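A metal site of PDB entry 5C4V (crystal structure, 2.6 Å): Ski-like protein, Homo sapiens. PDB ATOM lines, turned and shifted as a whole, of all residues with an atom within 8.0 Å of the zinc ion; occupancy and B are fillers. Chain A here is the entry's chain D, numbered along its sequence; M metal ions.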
ATOM      1  N   LYS A  35      18.257  24.300 -11.972  1.00  0.00           N
ATOM      2  CA  LYS A  35      17.018  23.964 -11.293  1.00  0.00           C
ATOM      3  C   LYS A  35      16.736  22.502 -11.473  1.00  0.00           C
ATOM      4  O   LYS A  35      17.147  21.931 -12.478  1.00  0.00           O
ATOM      5  CB  LYS A  35      15.885  24.786 -11.890  1.00  0.00           C
ATOM      6  N   CYS A  36      16.037  21.890 -10.518  1.00  0.00           N
ATOM      7  CA  CYS A  36      15.619  20.500 -10.662  1.00  0.00           C
ATOM      8  C   CYS A  36      14.503  20.144  -9.695  1.00  0.00           C
ATOM      9  O   CYS A  36      14.565  20.437  -8.491  1.00  0.00           O
ATOM     10  CB  CYS A  36      16.800  19.525 -10.473  1.00  0.00           C
ATOM     11  SG  CYS A  36      16.517  17.906 -11.186  1.00  0.00           S
ATOM     12  N   GLN A  37      13.524  19.440 -10.252  1.00  0.00           N
ATOM     13  CA  GLN A  37      12.345  18.993  -9.557  1.00  0.00           C
ATOM     14  C   GLN A  37      12.452  17.474  -9.345  1.00  0.00           C
ATOM     15  O   GLN A  37      12.969  16.753 -10.202  1.00  0.00           O
ATOM     16  CB  GLN A  37      11.117  19.338 -10.381  1.00  0.00           C
ATOM     17  CG  GLN A  37      10.793  20.808 -10.396  1.00  0.00           C
ATOM     18  CD  GLN A  37       9.729  21.171 -11.413  1.00  0.00           C
ATOM     19  OE1 GLN A  37      10.060  21.262 -12.576  1.00  0.00           O
ATOM     20  NE2 GLN A  37       8.469  21.371 -11.019  1.00  0.00           N
ATOM     21  N   GLN A  54      13.947  11.100  -6.762  1.00  0.00           N
ATOM     22  CA  GLN A  54      13.967  10.794  -8.160  1.00  0.00           C
ATOM     23  C   GLN A  54      13.797  12.029  -9.016  1.00  0.00           C
ATOM     24  O   GLN A  54      12.756  12.660  -9.000  1.00  0.00           O
ATOM     25  CB  GLN A  54      12.802   9.868  -8.483  1.00  0.00           C
ATOM     26  CG  GLN A  54      13.011   9.112  -9.758  1.00  0.00           C
ATOM     27  CD  GLN A  54      11.827   8.265 -10.128  1.00  0.00           C
ATOM     28  OE1 GLN A  54      10.681   8.676  -9.950  1.00  0.00           O
ATOM     29  NE2 GLN A  54      12.094   7.083 -10.687  1.00  0.00           N
ATOM     30  N   CYS A  55      14.778  12.326  -9.850  1.00  0.00           N
ATOM     31  CA  CYS A  55      14.629  13.431 -10.809  1.00  0.00           C
ATOM     32  C   CYS A  55      13.452  13.151 -11.749  1.00  0.00           C
ATOM     33  O   CYS A  55      13.418  12.149 -12.438  1.00  0.00           O
ATOM     34  CB  CYS A  55      15.924  13.697 -11.604  1.00  0.00           C
ATOM     35  SG  CYS A  55      15.613  14.659 -13.091  1.00  0.00           S
ATOM     36  N   LEU A  56      12.500  14.081 -11.766  1.00  0.00           N
ATOM     37  CA  LEU A  56      11.327  13.971 -12.634  1.00  0.00           C
ATOM     38  C   LEU A  56      11.653  14.015 -14.133  1.00  0.00           C
ATOM     39  O   LEU A  56      10.759  13.774 -14.921  1.00  0.00           O
ATOM     40  CB  LEU A  56      10.338  15.081 -12.340  1.00  0.00           C
ATOM     41  CG  LEU A  56       9.882  15.337 -10.905  1.00  0.00           C
ATOM     42  CD1 LEU A  56       8.814  16.456 -10.940  1.00  0.00           C
ATOM     43  CD2 LEU A  56       9.393  14.084 -10.190  1.00  0.00           C
ATOM     44  N   GLU A  57      12.880  14.367 -14.517  1.00  0.00           N
ATOM     45  CA  GLU A  57      13.233  14.453 -15.931  1.00  0.00           C
ATOM     46  C   GLU A  57      13.903  13.192 -16.442  1.00  0.00           C
ATOM     47  O   GLU A  57      13.534  12.698 -17.487  1.00  0.00           O
ATOM     48  CB  GLU A  57      14.178  15.628 -16.181  1.00  0.00           C
ATOM     49  CG  GLU A  57      13.483  16.953 -16.474  1.00  0.00           C
ATOM     50  CD  GLU A  57      14.486  17.950 -17.025  1.00  0.00           C
ATOM     51  OE1 GLU A  57      14.730  18.968 -16.368  1.00  0.00           O
ATOM     52  OE2 GLU A  57      15.085  17.697 -18.085  1.00  0.00           O
ATOM     53  N   CYS A  58      14.941  12.729 -15.732  1.00  0.00           N
ATOM     54  CA  CYS A  58      15.700  11.554 -16.120  1.00  0.00           C
ATOM     55  C   CYS A  58      15.319  10.293 -15.354  1.00  0.00           C
ATOM     56  O   CYS A  58      15.853   9.225 -15.633  1.00  0.00           O
ATOM     57  CB  CYS A  58      17.217  11.799 -15.953  1.00  0.00           C
ATOM     58  SG  CYS A  58      17.804  12.193 -14.275  1.00  0.00           S
ATOM     59  N   CYS A  59      14.450  10.414 -14.360  1.00  0.00           N
ATOM     60  CA  CYS A  59      14.010   9.298 -13.500  1.00  0.00           C
ATOM     61  C   CYS A  59      15.111   8.658 -12.666  1.00  0.00           C
ATOM     62  O   CYS A  59      14.936   7.563 -12.180  1.00  0.00           O
ATOM     63  CB  CYS A  59      13.253   8.249 -14.342  1.00  0.00           C
ATOM     64  SG  CYS A  59      11.957   9.019 -15.344  1.00  0.00           S
ATOM     65  N   GLY A  60      16.247   9.318 -12.496  1.00  0.00           N
ATOM     66  CA  GLY A  60      17.351   8.746 -11.725  1.00  0.00           C
ATOM     67  C   GLY A  60      17.129   9.014 -10.266  1.00  0.00           C
ATOM     68  O   GLY A  60      16.532  10.030  -9.909  1.00  0.00           O
ATOM     69  N   MET A  61      17.638   8.123  -9.437  1.00  0.00           N
ATOM     70  CA  MET A  61      17.485   8.185  -7.994  1.00  0.00           C
ATOM     71  C   MET A  61      18.742   8.767  -7.366  1.00  0.00           C
ATOM     72  O   MET A  61      19.815   8.195  -7.512  1.00  0.00           O
ATOM     73  CB  MET A  61      17.264   6.781  -7.408  1.00  0.00           C
ATOM     74  CG  MET A  61      16.019   6.046  -7.889  1.00  0.00           C
ATOM     75  SD  MET A  61      14.509   6.845  -7.285  1.00  0.00           S
ATOM     76  CE  MET A  61      14.747   6.723  -5.506  1.00  0.00           C
ATOM     77  N   PHE A  62      18.598   9.844  -6.591  1.00  0.00           N
ATOM     78  CA  PHE A  62      19.726  10.514  -5.965  1.00  0.00           C
ATOM     79  C   PHE A  62      19.616  10.609  -4.448  1.00  0.00           C
ATOM     80  O   PHE A  62      18.520  10.810  -3.894  1.00  0.00           O
ATOM     81  CB  PHE A  62      19.805  11.939  -6.506  1.00  0.00           C
ATOM     82  CG  PHE A  62      20.009  12.005  -7.986  1.00  0.00           C
ATOM     83  CD1 PHE A  62      18.901  11.910  -8.868  1.00  0.00           C
ATOM     84  CD2 PHE A  62      21.278  12.137  -8.512  1.00  0.00           C
ATOM     85  CE1 PHE A  62      19.078  11.956 -10.239  1.00  0.00           C
ATOM     86  CE2 PHE A  62      21.454  12.193  -9.893  1.00  0.00           C
ATOM     87  CZ  PHE A  62      20.361  12.116 -10.747  1.00  0.00           C
ATOM     88  N   PHE A  67      21.514  15.174  -5.255  1.00  0.00           N
ATOM     89  CA  PHE A  67      20.358  15.762  -5.980  1.00  0.00           C
ATOM     90  C   PHE A  67      20.573  17.268  -6.155  1.00  0.00           C
ATOM     91  O   PHE A  67      20.285  17.854  -7.204  1.00  0.00           O
ATOM     92  CB  PHE A  67      19.058  15.505  -5.216  1.00  0.00           C
ATOM     93  CG  PHE A  67      17.833  16.061  -5.904  1.00  0.00           C
ATOM     94  CD1 PHE A  67      17.446  15.584  -7.159  1.00  0.00           C
ATOM     95  CD2 PHE A  67      17.062  17.025  -5.304  1.00  0.00           C
ATOM     96  CE1 PHE A  67      16.309  16.075  -7.805  1.00  0.00           C
ATOM     97  CE2 PHE A  67      15.915  17.522  -5.930  1.00  0.00           C
ATOM     98  CZ  PHE A  67      15.528  17.045  -7.186  1.00  0.00           C
ATOM     99  N   HIS A  70      22.412  18.148  -9.078  1.00  0.00           N
ATOM    100  CA  HIS A  70      21.909  17.548 -10.316  1.00  0.00           C
ATOM    101  C   HIS A  70      20.963  18.526 -10.945  1.00  0.00           C
ATOM    102  O   HIS A  70      19.906  18.833 -10.376  1.00  0.00           O
ATOM    103  CB  HIS A  70      21.195  16.189 -10.035  1.00  0.00           C
ATOM    104  CG  HIS A  70      20.516  15.571 -11.227  1.00  0.00           C
ATOM    105  ND1 HIS A  70      21.182  15.151 -12.355  1.00  0.00           N
ATOM    106  CD2 HIS A  70      19.214  15.220 -11.425  1.00  0.00           C
ATOM    107  CE1 HIS A  70      20.320  14.615 -13.208  1.00  0.00           C
ATOM    108  NE2 HIS A  70      19.123  14.641 -12.654  1.00  0.00           N
ATOM    109  N   SER A  71      21.328  18.948 -12.149  1.00  0.00           N
ATOM    110  CA  SER A  71      20.495  19.843 -12.992  1.00  0.00           C
ATOM    111  C   SER A  71      20.699  19.493 -14.475  1.00  0.00           C
ATOM    112  O   SER A  71      21.801  19.262 -14.883  1.00  0.00           O
ATOM    113  CB  SER A  71      20.898  21.303 -12.769  1.00  0.00           C
ATOM    114  OG  SER A  71      20.633  22.120 -13.914  1.00  0.00           O
ATOM    115  N   HIS A  72      19.642  19.507 -15.266  1.00  0.00           N
ATOM    116  CA  HIS A  72      19.740  19.336 -16.727  1.00  0.00           C
ATOM    117  C   HIS A  72      19.941  20.628 -17.508  1.00  0.00           C
ATOM    118  O   HIS A  72      20.040  20.593 -18.724  1.00  0.00           O
ATOM    119  CB  HIS A  72      18.492  18.618 -17.263  1.00  0.00           C
ATOM    120  CG  HIS A  72      18.380  17.207 -16.817  1.00  0.00           C
ATOM    121  ND1 HIS A  72      17.330  16.392 -17.170  1.00  0.00           N
ATOM    122  CD2 HIS A  72      19.185  16.449 -16.020  1.00  0.00           C
ATOM    123  CE1 HIS A  72      17.503  15.196 -16.641  1.00  0.00           C
ATOM    124  NE2 HIS A  72      18.623  15.212 -15.932  1.00  0.00           N
HETATM  125 ZN    ZN M   1      17.574  14.371 -14.156  1.00  0.00          ZN
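Four residues have an atom within 4 Å of the zinc ion: Cys 55, Cys 58, His 70 and His 72.
The zinc ion is bound by a ring nitrogen (NE2) of His 70, the side-chain sulfur (SG) of Cys 58, a ring nitrogen (NE2) of His 72 and the side-chain sulfur (SG) of Cys 55. The zinc ion has four donor atoms within binding distance.
ND1 of His 72 lies within hydrogen-bond range of OE2 of Glu 57 (2.8 Å). SG of Cys 55 lies close to N of Glu 57, at 3.1 Å. The side-chain sulfur (SG) of Cys 36 sits close to the backbone carbonyl oxygen (O) of His 70 (3.6 Å). The backbone NH (N) of Cys 55 sits at hydrogen-bond distance from the backbone carbonyl oxygen (O) of Gly 60, 2.9 Å away. The side-chain sulfur (SG) of Cys 58 lies close to the backbone NH (N) of Gly 60, at 3.7 Å.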
